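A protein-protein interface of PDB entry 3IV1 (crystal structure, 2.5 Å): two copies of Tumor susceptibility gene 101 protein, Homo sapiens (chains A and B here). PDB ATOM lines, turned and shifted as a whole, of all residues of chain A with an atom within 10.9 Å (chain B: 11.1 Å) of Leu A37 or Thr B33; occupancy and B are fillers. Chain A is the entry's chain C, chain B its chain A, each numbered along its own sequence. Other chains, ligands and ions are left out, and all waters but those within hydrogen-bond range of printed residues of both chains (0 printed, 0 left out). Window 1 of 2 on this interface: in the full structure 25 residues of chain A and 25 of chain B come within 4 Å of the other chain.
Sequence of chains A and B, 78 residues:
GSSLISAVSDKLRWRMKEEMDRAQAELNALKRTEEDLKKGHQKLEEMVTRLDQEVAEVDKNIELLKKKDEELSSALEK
OE2 of Glu B26 lies within salt-bridge range of NZ of Lys A43, 3.6 Å away.
The backbone carbonyl oxygen (O) of Ala B29 sits at hydrogen-bond distance from the side-chain hydroxyl (OG1) of Thr B33 (3.2 Å).
O of Leu B37 lies close to ND1 of His B41 (3.3 Å).
OG1 of Thr A33 sits at hydrogen-bond distance from O of Ala A29, at 3.1 Å.
The guanidinium group (NH1) of Arg A32 lies within salt-bridge range of the side-chain carboxylate (OD1) of Asp A36, 2.8 Å away.
ND1 of His A41 lies close to O of Leu A37 (3.4 Å).
Among the printed residues, merely in contact across the chains: Glu A26 with Gly B40 (3.6 Å), Leu A30 with Leu B37 (3.8 Å), Leu A30 with His B41 (3.96 Å), Thr A33 with Thr B33 (3.4 Å), Thr A33 with Asp B36 (3.8 Å), Thr A33 with Leu B37 (3.7 Å), Asp A36 with Thr B33 (3.9 Å), Leu A37 with Leu B30 (3.9 Å), Leu A37 with Thr B33 (3.8 Å), Gly A40 with Glu B26 (3.2 Å), Gly A40 with Leu B30 (3.997 Å) and Leu A44 with Leu B30 (3.8 Å).
Leu A37 touches two residues of chain B.
Of chain A, only Thr A33 (3.4 Å), Asp A36 (3.9 Å) and Leu A37 (3.8 Å) come within 4 Å of Thr B33.
Of chain B, only Thr B33 (3.4 Å), Asp B36 (3.8 Å) and Leu B37 (3.7 Å) come within 4 Å of Thr A33.
Asp A36 touches just one residue of chain B: Thr B33 (3.9 Å).
Ala B29 touches none of the printed residues of chain A.
Of chain A, only Thr A33 comes within 4 Å of Asp B36.
Of the printed residues of chain A, Leu B37 touches Leu A30 (3.8 Å) and Thr A33 (3.7 Å).
Of the printed residues of chain B, Glu A26 touches Gly B40 (3.6 Å).
Printed residues of chain A within 4 Å of Glu B26: Gly A40 (3.2 Å) and Lys A43 (3.2 Å).
Of the printed residues of chain B, Leu A30 touches Leu B37 and His B41.
Printed residues of chain A within 4 Å of Gly B40: Glu A26.
Lys B39 touches none of the printed residues of chain A.
The nearest residue of chain B that does not touch Leu A37 is Leu B37 (4.8 Å).
The nearest printed residue of chain A that does not touch Glu B26 is Leu A44 (4.3 Å).
Of the 18 printed residues of chain B, 7 touch a printed residue of chain A.
Hydrophobic or aromatic side chains of chain B that line the printed part of chain A: Leu B30, Leu B37 and His B41.
Among the printed residues, 13 pairs touch across the chains.
Glu A26 touches Gly B40, and with the chains exchanged Gly A40 touches Glu B26.
Thr A33 touches Asp B36, and with the chains exchanged Asp A36 touches Thr B33.
Thr A33 touches Leu B37, and with the chains exchanged Leu A37 touches Thr B33.
Gly A40 touches Leu B30, but with the chains exchanged Leu A30 does not touch Gly B40 (4.1 Å).
Positions printed for both chains: 26, 29, 30, 31, 32, 33, 34, 35, 36, 37, 38, 39, 40, 41 and 42.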
ATOM      1  N   GLU A  26      -8.896 -40.990 -10.687  1.00  0.00           N
ATOM      2  CA  GLU A  26      -8.315 -40.281  -9.539  1.00  0.00           C
ATOM      3  C   GLU A  26      -6.784 -40.231  -9.628  1.00  0.00           C
ATOM      4  O   GLU A  26      -6.184 -39.186  -9.361  1.00  0.00           O
ATOM      5  CB  GLU A  26      -8.745 -40.931  -8.217  1.00  0.00           C
ATOM      6  CG  GLU A  26      -8.790 -39.967  -7.049  1.00  0.00           C
ATOM      7  CD  GLU A  26      -9.592 -38.693  -7.252  1.00  0.00           C
ATOM      8  OE1 GLU A  26     -10.820 -38.797  -7.484  1.00  0.00           O
ATOM      9  OE2 GLU A  26      -8.997 -37.592  -7.165  1.00  0.00           O
ATOM     10  N   ALA A  29      -5.627 -37.667 -12.348  1.00  0.00           N
ATOM     11  CA  ALA A  29      -5.724 -36.317 -11.782  1.00  0.00           C
ATOM     12  C   ALA A  29      -4.555 -36.059 -10.803  1.00  0.00           C
ATOM     13  O   ALA A  29      -4.014 -34.953 -10.765  1.00  0.00           O
ATOM     14  CB  ALA A  29      -7.065 -36.143 -11.073  1.00  0.00           C
ATOM     15  N   LEU A  30      -4.137 -37.096 -10.050  1.00  0.00           N
ATOM     16  CA  LEU A  30      -3.014 -37.002  -9.110  1.00  0.00           C
ATOM     17  C   LEU A  30      -1.675 -36.849  -9.798  1.00  0.00           C
ATOM     18  O   LEU A  30      -0.786 -36.250  -9.200  1.00  0.00           O
ATOM     19  CB  LEU A  30      -2.988 -38.160  -8.087  1.00  0.00           C
ATOM     20  CG  LEU A  30      -4.008 -38.062  -6.949  1.00  0.00           C
ATOM     21  CD1 LEU A  30      -4.220 -39.417  -6.286  1.00  0.00           C
ATOM     22  CD2 LEU A  30      -3.615 -36.990  -5.928  1.00  0.00           C
ATOM     23  N   LYS A  31      -1.530 -37.325 -11.053  1.00  0.00           N
ATOM     24  CA  LYS A  31      -0.279 -37.194 -11.808  1.00  0.00           C
ATOM     25  C   LYS A  31      -0.063 -35.755 -12.265  1.00  0.00           C
ATOM     26  O   LYS A  31       1.079 -35.311 -12.369  1.00  0.00           O
ATOM     27  CB  LYS A  31      -0.201 -38.174 -12.995  1.00  0.00           C
ATOM     28  CG  LYS A  31      -0.092 -39.637 -12.550  1.00  0.00           C
ATOM     29  CD  LYS A  31       0.596 -40.540 -13.585  1.00  0.00           C
ATOM     30  CE  LYS A  31      -0.293 -40.994 -14.724  1.00  0.00           C
ATOM     31  NZ  LYS A  31      -1.459 -41.778 -14.246  1.00  0.00           N
ATOM     32  N   ARG A  32      -1.160 -35.035 -12.533  1.00  0.00           N
ATOM     33  CA  ARG A  32      -1.145 -33.624 -12.901  1.00  0.00           C
ATOM     34  C   ARG A  32      -0.776 -32.807 -11.638  1.00  0.00           C
ATOM     35  O   ARG A  32      -0.016 -31.843 -11.728  1.00  0.00           O
ATOM     36  CB  ARG A  32      -2.517 -33.211 -13.471  1.00  0.00           C
ATOM     37  CG  ARG A  32      -2.703 -31.710 -13.711  1.00  0.00           C
ATOM     38  CD  ARG A  32      -2.453 -31.311 -15.156  1.00  0.00           C
ATOM     39  NE  ARG A  32      -2.621 -29.870 -15.362  1.00  0.00           N
ATOM     40  CZ  ARG A  32      -1.648 -28.976 -15.217  1.00  0.00           C
ATOM     41  NH1 ARG A  32      -0.427 -29.362 -14.865  1.00  0.00           N
ATOM     42  NH2 ARG A  32      -1.890 -27.687 -15.417  1.00  0.00           N
ATOM     43  N   THR A  33      -1.288 -33.231 -10.463  1.00  0.00           N
ATOM     44  CA  THR A  33      -0.992 -32.624  -9.172  1.00  0.00           C
ATOM     45  C   THR A  33       0.503 -32.807  -8.846  1.00  0.00           C
ATOM     46  O   THR A  33       1.135 -31.856  -8.380  1.00  0.00           O
ATOM     47  CB  THR A  33      -1.974 -33.156  -8.106  1.00  0.00           C
ATOM     48  OG1 THR A  33      -3.310 -32.901  -8.538  1.00  0.00           O
ATOM     49  CG2 THR A  33      -1.775 -32.518  -6.740  1.00  0.00           C
ATOM     50  N   GLU A  34       1.083 -34.003  -9.154  1.00  0.00           N
ATOM     51  CA  GLU A  34       2.522 -34.272  -8.946  1.00  0.00           C
ATOM     52  C   GLU A  34       3.348 -33.300  -9.791  1.00  0.00           C
ATOM     53  O   GLU A  34       4.369 -32.806  -9.328  1.00  0.00           O
ATOM     54  CB  GLU A  34       2.922 -35.679  -9.433  1.00  0.00           C
ATOM     55  CG  GLU A  34       2.370 -36.880  -8.703  1.00  0.00           C
ATOM     56  CD  GLU A  34       2.550 -38.169  -9.488  1.00  0.00           C
ATOM     57  OE1 GLU A  34       2.827 -38.111 -10.709  1.00  0.00           O
ATOM     58  OE2 GLU A  34       2.415 -39.250  -8.876  1.00  0.00           O
ATOM     59  N   GLU A  35       2.938 -33.104 -11.057  1.00  0.00           N
ATOM     60  CA  GLU A  35       3.573 -32.216 -12.024  1.00  0.00           C
ATOM     61  C   GLU A  35       3.565 -30.756 -11.512  1.00  0.00           C
ATOM     62  O   GLU A  35       4.603 -30.107 -11.571  1.00  0.00           O
ATOM     63  CB  GLU A  35       2.895 -32.359 -13.403  1.00  0.00           C
ATOM     64  CG  GLU A  35       3.364 -31.372 -14.459  1.00  0.00           C
ATOM     65  CD  GLU A  35       2.345 -31.069 -15.547  1.00  0.00           C
ATOM     66  OE1 GLU A  35       1.766 -32.024 -16.115  1.00  0.00           O
ATOM     67  OE2 GLU A  35       2.141 -29.867 -15.839  1.00  0.00           O
ATOM     68  N   ASP A  36       2.426 -30.269 -10.975  1.00  0.00           N
ATOM     69  CA  ASP A  36       2.327 -28.921 -10.404  1.00  0.00           C
ATOM     70  C   ASP A  36       3.266 -28.752  -9.201  1.00  0.00           C
ATOM     71  O   ASP A  36       3.821 -27.672  -9.007  1.00  0.00           O
ATOM     72  CB  ASP A  36       0.889 -28.602  -9.981  1.00  0.00           C
ATOM     73  CG  ASP A  36      -0.103 -28.446 -11.119  1.00  0.00           C
ATOM     74  OD1 ASP A  36       0.336 -28.409 -12.296  1.00  0.00           O
ATOM     75  OD2 ASP A  36      -1.322 -28.348 -10.836  1.00  0.00           O
ATOM     76  N   LEU A  37       3.457 -29.835  -8.424  1.00  0.00           N
ATOM     77  CA  LEU A  37       4.326 -29.878  -7.253  1.00  0.00           C
ATOM     78  C   LEU A  37       5.804 -29.769  -7.635  1.00  0.00           C
ATOM     79  O   LEU A  37       6.531 -28.994  -7.000  1.00  0.00           O
ATOM     80  CB  LEU A  37       4.057 -31.155  -6.472  1.00  0.00           C
ATOM     81  CG  LEU A  37       4.485 -31.158  -5.028  1.00  0.00           C
ATOM     82  CD1 LEU A  37       3.516 -30.354  -4.168  1.00  0.00           C
ATOM     83  CD2 LEU A  37       4.596 -32.571  -4.524  1.00  0.00           C
ATOM     84  N   LYS A  38       6.234 -30.542  -8.662  1.00  0.00           N
ATOM     85  CA  LYS A  38       7.612 -30.548  -9.182  1.00  0.00           C
ATOM     86  C   LYS A  38       7.953 -29.145  -9.691  1.00  0.00           C
ATOM     87  O   LYS A  38       8.952 -28.575  -9.262  1.00  0.00           O
ATOM     88  CB  LYS A  38       7.770 -31.560 -10.339  1.00  0.00           C
ATOM     89  CG  LYS A  38       9.051 -32.402 -10.329  1.00  0.00           C
ATOM     90  CD  LYS A  38      10.381 -31.656 -10.182  1.00  0.00           C
ATOM     91  CE  LYS A  38      11.559 -32.605 -10.115  1.00  0.00           C
ATOM     92  NZ  LYS A  38      12.855 -31.877 -10.119  1.00  0.00           N
ATOM     93  N   LYS A  39       7.081 -28.590 -10.564  1.00  0.00           N
ATOM     94  CA  LYS A  39       7.167 -27.259 -11.172  1.00  0.00           C
ATOM     95  C   LYS A  39       7.345 -26.169 -10.091  1.00  0.00           C
ATOM     96  O   LYS A  39       8.249 -25.339 -10.210  1.00  0.00           O
ATOM     97  CB  LYS A  39       5.902 -26.999 -12.006  1.00  0.00           C
ATOM     98  CG  LYS A  39       6.162 -26.466 -13.405  1.00  0.00           C
ATOM     99  CD  LYS A  39       4.938 -26.591 -14.326  1.00  0.00           C
ATOM    100  CE  LYS A  39       3.990 -25.408 -14.265  1.00  0.00           C
ATOM    101  NZ  LYS A  39       2.945 -25.490 -15.321  1.00  0.00           N
ATOM    102  N   GLY A  40       6.523 -26.218  -9.040  1.00  0.00           N
ATOM    103  CA  GLY A  40       6.577 -25.271  -7.928  1.00  0.00           C
ATOM    104  C   GLY A  40       7.903 -25.286  -7.189  1.00  0.00           C
ATOM    105  O   GLY A  40       8.470 -24.229  -6.903  1.00  0.00           O
ATOM    106  N   HIS A  41       8.430 -26.504  -6.931  1.00  0.00           N
ATOM    107  CA  HIS A  41       9.709 -26.720  -6.269  1.00  0.00           C
ATOM    108  C   HIS A  41      10.878 -26.248  -7.147  1.00  0.00           C
ATOM    109  O   HIS A  41      11.834 -25.657  -6.640  1.00  0.00           O
ATOM    110  CB  HIS A  41       9.852 -28.203  -5.854  1.00  0.00           C
ATOM    111  CG  HIS A  41       8.880 -28.626  -4.788  1.00  0.00           C
ATOM    112  ND1 HIS A  41       8.627 -29.953  -4.540  1.00  0.00           N
ATOM    113  CD2 HIS A  41       8.134 -27.879  -3.941  1.00  0.00           C
ATOM    114  CE1 HIS A  41       7.754 -29.970  -3.556  1.00  0.00           C
ATOM    115  NE2 HIS A  41       7.415 -28.746  -3.182  1.00  0.00           N
ATOM    116  N   GLN A  42      10.770 -26.477  -8.456  1.00  0.00           N
ATOM    117  CA  GLN A  42      11.765 -26.070  -9.450  1.00  0.00           C
ATOM    118  C   GLN A  42      11.864 -24.542  -9.520  1.00  0.00           C
ATOM    119  O   GLN A  42      12.972 -24.006  -9.491  1.00  0.00           O
ATOM    120  CB  GLN A  42      11.439 -26.668 -10.819  1.00  0.00           C
ATOM    121  CG  GLN A  42      11.813 -28.149 -10.944  1.00  0.00           C
ATOM    122  CD  GLN A  42      11.476 -28.762 -12.297  1.00  0.00           C
ATOM    123  OE1 GLN A  42      10.784 -28.174 -13.152  1.00  0.00           O
ATOM    124  NE2 GLN A  42      11.959 -29.978 -12.519  1.00  0.00           N
ATOM    125  N   LYS A  43      10.703 -23.844  -9.546  1.00  0.00           N
ATOM    126  CA  LYS A  43      10.627 -22.385  -9.548  1.00  0.00           C
ATOM    127  C   LYS A  43      11.277 -21.834  -8.289  1.00  0.00           C
ATOM    128  O   LYS A  43      12.084 -20.914  -8.391  1.00  0.00           O
ATOM    129  CB  LYS A  43       9.179 -21.878  -9.715  1.00  0.00           C
ATOM    130  CG  LYS A  43       8.627 -22.114 -11.116  1.00  0.00           C
ATOM    131  CD  LYS A  43       7.441 -21.241 -11.429  1.00  0.00           C
ATOM    132  CE  LYS A  43       6.672 -21.738 -12.628  1.00  0.00           C
ATOM    133  NZ  LYS A  43       5.486 -20.883 -12.909  1.00  0.00           N
ATOM    134  N   LEU A  44      10.995 -22.438  -7.119  1.00  0.00           N
ATOM    135  CA  LEU A  44      11.610 -22.023  -5.853  1.00  0.00           C
ATOM    136  C   LEU A  44      13.133 -22.224  -5.845  1.00  0.00           C
ATOM    137  O   LEU A  44      13.859 -21.337  -5.401  1.00  0.00           O
ATOM    138  CB  LEU A  44      10.960 -22.704  -4.657  1.00  0.00           C
ATOM    139  CG  LEU A  44       9.548 -22.223  -4.302  1.00  0.00           C
ATOM    140  CD1 LEU A  44       8.852 -23.221  -3.375  1.00  0.00           C
ATOM    141  CD2 LEU A  44       9.575 -20.791  -3.692  1.00  0.00           C
ATOM    142  N   GLU A  45      13.608 -23.347  -6.399  1.00  0.00           N
ATOM    143  CA  GLU A  45      15.045 -23.652  -6.505  1.00  0.00           C
ATOM    144  C   GLU A  45      15.760 -22.653  -7.441  1.00  0.00           C
ATOM    145  O   GLU A  45      16.848 -22.176  -7.109  1.00  0.00           O
ATOM    146  CB  GLU A  45      15.248 -25.104  -6.936  1.00  0.00           C
ATOM    147  CG  GLU A  45      16.677 -25.597  -6.805  1.00  0.00           C
ATOM    148  CD  GLU A  45      16.787 -27.108  -6.848  1.00  0.00           C
ATOM    149  OE1 GLU A  45      16.544 -27.694  -7.927  1.00  0.00           O
ATOM    150  OE2 GLU A  45      17.052 -27.713  -5.785  1.00  0.00           O
ATOM    151  N   ALA B  25       3.818 -16.148  -3.876  1.00  0.00           N
ATOM    152  CA  ALA B  25       2.816 -16.554  -4.870  1.00  0.00           C
ATOM    153  C   ALA B  25       2.994 -18.041  -5.222  1.00  0.00           C
ATOM    154  O   ALA B  25       2.000 -18.754  -5.273  1.00  0.00           O
ATOM    155  CB  ALA B  25       2.920 -15.690  -6.122  1.00  0.00           C
ATOM    156  N   GLU B  26       4.257 -18.520  -5.397  1.00  0.00           N
ATOM    157  CA  GLU B  26       4.542 -19.933  -5.687  1.00  0.00           C
ATOM    158  C   GLU B  26       4.106 -20.832  -4.526  1.00  0.00           C
ATOM    159  O   GLU B  26       3.500 -21.878  -4.754  1.00  0.00           O
ATOM    160  CB  GLU B  26       6.035 -20.177  -5.992  1.00  0.00           C
ATOM    161  CG  GLU B  26       6.360 -20.454  -7.460  1.00  0.00           C
ATOM    162  CD  GLU B  26       5.429 -21.370  -8.237  1.00  0.00           C
ATOM    163  OE1 GLU B  26       5.104 -22.474  -7.739  1.00  0.00           O
ATOM    164  OE2 GLU B  26       4.999 -20.964  -9.340  1.00  0.00           O
ATOM    165  N   LEU B  27       4.389 -20.405  -3.281  1.00  0.00           N
ATOM    166  CA  LEU B  27       3.996 -21.126  -2.071  1.00  0.00           C
ATOM    167  C   LEU B  27       2.470 -21.170  -1.871  1.00  0.00           C
ATOM    168  O   LEU B  27       1.953 -22.215  -1.480  1.00  0.00           O
ATOM    169  CB  LEU B  27       4.730 -20.600  -0.838  1.00  0.00           C
ATOM    170  CG  LEU B  27       6.197 -21.025  -0.766  1.00  0.00           C
ATOM    171  CD1 LEU B  27       7.009 -20.054   0.069  1.00  0.00           C
ATOM    172  CD2 LEU B  27       6.341 -22.501  -0.312  1.00  0.00           C
ATOM    173  N   ASN B  28       1.755 -20.086  -2.236  1.00  0.00           N
ATOM    174  CA  ASN B  28       0.290 -20.059  -2.157  1.00  0.00           C
ATOM    175  C   ASN B  28      -0.316 -21.086  -3.125  1.00  0.00           C
ATOM    176  O   ASN B  28      -1.242 -21.791  -2.736  1.00  0.00           O
ATOM    177  CB  ASN B  28      -0.263 -18.662  -2.472  1.00  0.00           C
ATOM    178  CG  ASN B  28      -0.040 -17.593  -1.431  1.00  0.00           C
ATOM    179  OD1 ASN B  28      -0.152 -16.401  -1.730  1.00  0.00           O
ATOM    180  ND2 ASN B  28       0.126 -17.964  -0.174  1.00  0.00           N
ATOM    181  N   ALA B  29       0.234 -21.188  -4.366  1.00  0.00           N
ATOM    182  CA  ALA B  29      -0.192 -22.147  -5.394  1.00  0.00           C
ATOM    183  C   ALA B  29       0.121 -23.578  -4.944  1.00  0.00           C
ATOM    184  O   ALA B  29      -0.683 -24.483  -5.185  1.00  0.00           O
ATOM    185  CB  ALA B  29       0.493 -21.843  -6.716  1.00  0.00           C
ATOM    186  N   LEU B  30       1.251 -23.777  -4.232  1.00  0.00           N
ATOM    187  CA  LEU B  30       1.643 -25.086  -3.690  1.00  0.00           C
ATOM    188  C   LEU B  30       0.735 -25.548  -2.554  1.00  0.00           C
ATOM    189  O   LEU B  30       0.586 -26.733  -2.379  1.00  0.00           O
ATOM    190  CB  LEU B  30       3.128 -25.131  -3.288  1.00  0.00           C
ATOM    191  CG  LEU B  30       4.130 -25.241  -4.449  1.00  0.00           C
ATOM    192  CD1 LEU B  30       5.525 -24.840  -4.000  1.00  0.00           C
ATOM    193  CD2 LEU B  30       4.121 -26.636  -5.085  1.00  0.00           C
ATOM    194  N   LYS B  31       0.100 -24.635  -1.828  1.00  0.00           N
ATOM    195  CA  LYS B  31      -0.869 -24.951  -0.758  1.00  0.00           C
ATOM    196  C   LYS B  31      -2.144 -25.554  -1.361  1.00  0.00           C
ATOM    197  O   LYS B  31      -2.734 -26.448  -0.770  1.00  0.00           O
ATOM    198  CB  LYS B  31      -1.223 -23.703   0.097  1.00  0.00           C
ATOM    199  CG  LYS B  31      -0.040 -23.179   0.917  1.00  0.00           C
ATOM    200  CD  LYS B  31      -0.282 -23.140   2.419  1.00  0.00           C
ATOM    201  CE  LYS B  31       1.010 -23.254   3.218  1.00  0.00           C
ATOM    202  NZ  LYS B  31       1.330 -24.667   3.591  1.00  0.00           N
ATOM    203  N   ARG B  32      -2.572 -25.050  -2.530  1.00  0.00           N
ATOM    204  CA  ARG B  32      -3.734 -25.567  -3.248  1.00  0.00           C
ATOM    205  C   ARG B  32      -3.436 -26.945  -3.852  1.00  0.00           C
ATOM    206  O   ARG B  32      -4.308 -27.806  -3.824  1.00  0.00           O
ATOM    207  CB  ARG B  32      -4.194 -24.566  -4.307  1.00  0.00           C
ATOM    208  CG  ARG B  32      -5.189 -23.539  -3.757  1.00  0.00           C
ATOM    209  CD  ARG B  32      -4.525 -22.282  -3.208  1.00  0.00           C
ATOM    210  NE  ARG B  32      -5.511 -21.357  -2.645  1.00  0.00           N
ATOM    211  CZ  ARG B  32      -5.225 -20.155  -2.154  1.00  0.00           C
ATOM    212  NH1 ARG B  32      -3.975 -19.708  -2.156  1.00  0.00           N
ATOM    213  NH2 ARG B  32      -6.186 -19.393  -1.650  1.00  0.00           N
ATOM    214  N   THR B  33      -2.187 -27.166  -4.347  1.00  0.00           N
ATOM    215  CA  THR B  33      -1.696 -28.447  -4.856  1.00  0.00           C
ATOM    216  C   THR B  33      -1.679 -29.486  -3.690  1.00  0.00           C
ATOM    217  O   THR B  33      -2.090 -30.640  -3.874  1.00  0.00           O
ATOM    218  CB  THR B  33      -0.299 -28.266  -5.494  1.00  0.00           C
ATOM    219  OG1 THR B  33      -0.374 -27.318  -6.557  1.00  0.00           O
ATOM    220  CG2 THR B  33       0.286 -29.565  -6.034  1.00  0.00           C
ATOM    221  N   GLU B  34      -1.232 -29.069  -2.496  1.00  0.00           N
ATOM    222  CA  GLU B  34      -1.191 -29.969  -1.345  1.00  0.00           C
ATOM    223  C   GLU B  34      -2.621 -30.358  -0.862  1.00  0.00           C
ATOM    224  O   GLU B  34      -2.844 -31.489  -0.430  1.00  0.00           O
ATOM    225  CB  GLU B  34      -0.216 -29.456  -0.246  1.00  0.00           C
ATOM    226  CG  GLU B  34      -0.795 -28.463   0.742  1.00  0.00           C
ATOM    227  CD  GLU B  34       0.174 -27.704   1.634  1.00  0.00           C
ATOM    228  OE1 GLU B  34       1.344 -27.494   1.236  1.00  0.00           O
ATOM    229  OE2 GLU B  34      -0.274 -27.250   2.712  1.00  0.00           O
ATOM    230  N   GLU B  35      -3.605 -29.463  -1.068  1.00  0.00           N
ATOM    231  CA  GLU B  35      -5.006 -29.739  -0.776  1.00  0.00           C
ATOM    232  C   GLU B  35      -5.579 -30.748  -1.779  1.00  0.00           C
ATOM    233  O   GLU B  35      -6.381 -31.585  -1.389  1.00  0.00           O
ATOM    234  CB  GLU B  35      -5.841 -28.454  -0.769  1.00  0.00           C
ATOM    235  CG  GLU B  35      -5.640 -27.610   0.479  1.00  0.00           C
ATOM    236  CD  GLU B  35      -6.575 -26.421   0.584  1.00  0.00           C
ATOM    237  OE1 GLU B  35      -6.093 -25.274   0.435  1.00  0.00           O
ATOM    238  OE2 GLU B  35      -7.788 -26.630   0.820  1.00  0.00           O
ATOM    239  N   ASP B  36      -5.167 -30.675  -3.054  1.00  0.00           N
ATOM    240  CA  ASP B  36      -5.615 -31.594  -4.112  1.00  0.00           C
ATOM    241  C   ASP B  36      -5.120 -33.024  -3.892  1.00  0.00           C
ATOM    242  O   ASP B  36      -5.835 -33.987  -4.192  1.00  0.00           O
ATOM    243  CB  ASP B  36      -5.108 -31.110  -5.477  1.00  0.00           C
ATOM    244  CG  ASP B  36      -5.800 -29.881  -6.008  1.00  0.00           C
ATOM    245  OD1 ASP B  36      -6.726 -29.386  -5.336  1.00  0.00           O
ATOM    246  OD2 ASP B  36      -5.440 -29.434  -7.116  1.00  0.00           O
ATOM    247  N   LEU B  37      -3.871 -33.143  -3.398  1.00  0.00           N
ATOM    248  CA  LEU B  37      -3.177 -34.392  -3.118  1.00  0.00           C
ATOM    249  C   LEU B  37      -3.882 -35.142  -1.998  1.00  0.00           C
ATOM    250  O   LEU B  37      -4.144 -36.338  -2.140  1.00  0.00           O
ATOM    251  CB  LEU B  37      -1.748 -34.046  -2.719  1.00  0.00           C
ATOM    252  CG  LEU B  37      -0.631 -35.003  -3.045  1.00  0.00           C
ATOM    253  CD1 LEU B  37      -0.488 -35.234  -4.580  1.00  0.00           C
ATOM    254  CD2 LEU B  37       0.665 -34.449  -2.480  1.00  0.00           C
ATOM    255  N   LYS B  38      -4.254 -34.408  -0.925  1.00  0.00           N
ATOM    256  CA  LYS B  38      -4.955 -34.870   0.266  1.00  0.00           C
ATOM    257  C   LYS B  38      -6.329 -35.413  -0.149  1.00  0.00           C
ATOM    258  O   LYS B  38      -6.616 -36.587   0.109  1.00  0.00           O
ATOM    259  CB  LYS B  38      -5.075 -33.699   1.258  1.00  0.00           C
ATOM    260  CG  LYS B  38      -5.606 -34.039   2.652  1.00  0.00           C
ATOM    261  CD  LYS B  38      -4.993 -33.119   3.724  1.00  0.00           C
ATOM    262  CE  LYS B  38      -5.571 -31.714   3.762  1.00  0.00           C
ATOM    263  NZ  LYS B  38      -4.534 -30.691   4.087  1.00  0.00           N
ATOM    264  N   LYS B  39      -7.142 -34.575  -0.851  1.00  0.00           N
ATOM    265  CA  LYS B  39      -8.468 -34.925  -1.383  1.00  0.00           C
ATOM    266  C   LYS B  39      -8.413 -36.200  -2.237  1.00  0.00           C
ATOM    267  O   LYS B  39      -9.234 -37.106  -2.024  1.00  0.00           O
ATOM    268  CB  LYS B  39      -9.070 -33.779  -2.196  1.00  0.00           C
ATOM    269  CG  LYS B  39      -9.602 -32.669  -1.338  1.00  0.00           C
ATOM    270  CD  LYS B  39     -10.320 -31.636  -2.176  1.00  0.00           C
ATOM    271  CE  LYS B  39     -10.324 -30.329  -1.452  1.00  0.00           C
ATOM    272  NZ  LYS B  39     -11.098 -29.305  -2.195  1.00  0.00           N
ATOM    273  N   GLY B  40      -7.420 -36.278  -3.140  1.00  0.00           N
ATOM    274  CA  GLY B  40      -7.210 -37.421  -4.025  1.00  0.00           C
ATOM    275  C   GLY B  40      -6.910 -38.703  -3.274  1.00  0.00           C
ATOM    276  O   GLY B  40      -7.465 -39.753  -3.580  1.00  0.00           O
ATOM    277  N   HIS B  41      -6.058 -38.608  -2.253  1.00  0.00           N
ATOM    278  CA  HIS B  41      -5.687 -39.724  -1.387  1.00  0.00           C
ATOM    279  C   HIS B  41      -6.861 -40.150  -0.522  1.00  0.00           C
ATOM    280  O   HIS B  41      -7.043 -41.342  -0.316  1.00  0.00           O
ATOM    281  CB  HIS B  41      -4.460 -39.372  -0.521  1.00  0.00           C
ATOM    282  CG  HIS B  41      -3.194 -39.183  -1.305  1.00  0.00           C
ATOM    283  ND1 HIS B  41      -2.113 -38.531  -0.765  1.00  0.00           N
ATOM    284  CD2 HIS B  41      -2.881 -39.576  -2.559  1.00  0.00           C
ATOM    285  CE1 HIS B  41      -1.174 -38.557  -1.695  1.00  0.00           C
ATOM    286  NE2 HIS B  41      -1.592 -39.168  -2.794  1.00  0.00           N
ATOM    287  N   GLN B  42      -7.673 -39.195  -0.060  1.00  0.00           N
ATOM    288  CA  GLN B  42      -8.846 -39.458   0.770  1.00  0.00           C
ATOM    289  C   GLN B  42      -9.903 -40.240  -0.002  1.00  0.00           C
ATOM    290  O   GLN B  42     -10.409 -41.246   0.506  1.00  0.00           O
ATOM    291  CB  GLN B  42      -9.425 -38.154   1.341  1.00  0.00           C
ATOM    292  CG  GLN B  42      -8.629 -37.606   2.525  1.00  0.00           C
ATOM    293  CD  GLN B  42      -9.181 -36.315   3.081  1.00  0.00           C
ATOM    294  OE1 GLN B  42     -10.026 -35.634   2.479  1.00  0.00           O
ATOM    295  NE2 GLN B  42      -8.698 -35.940   4.250  1.00  0.00           N
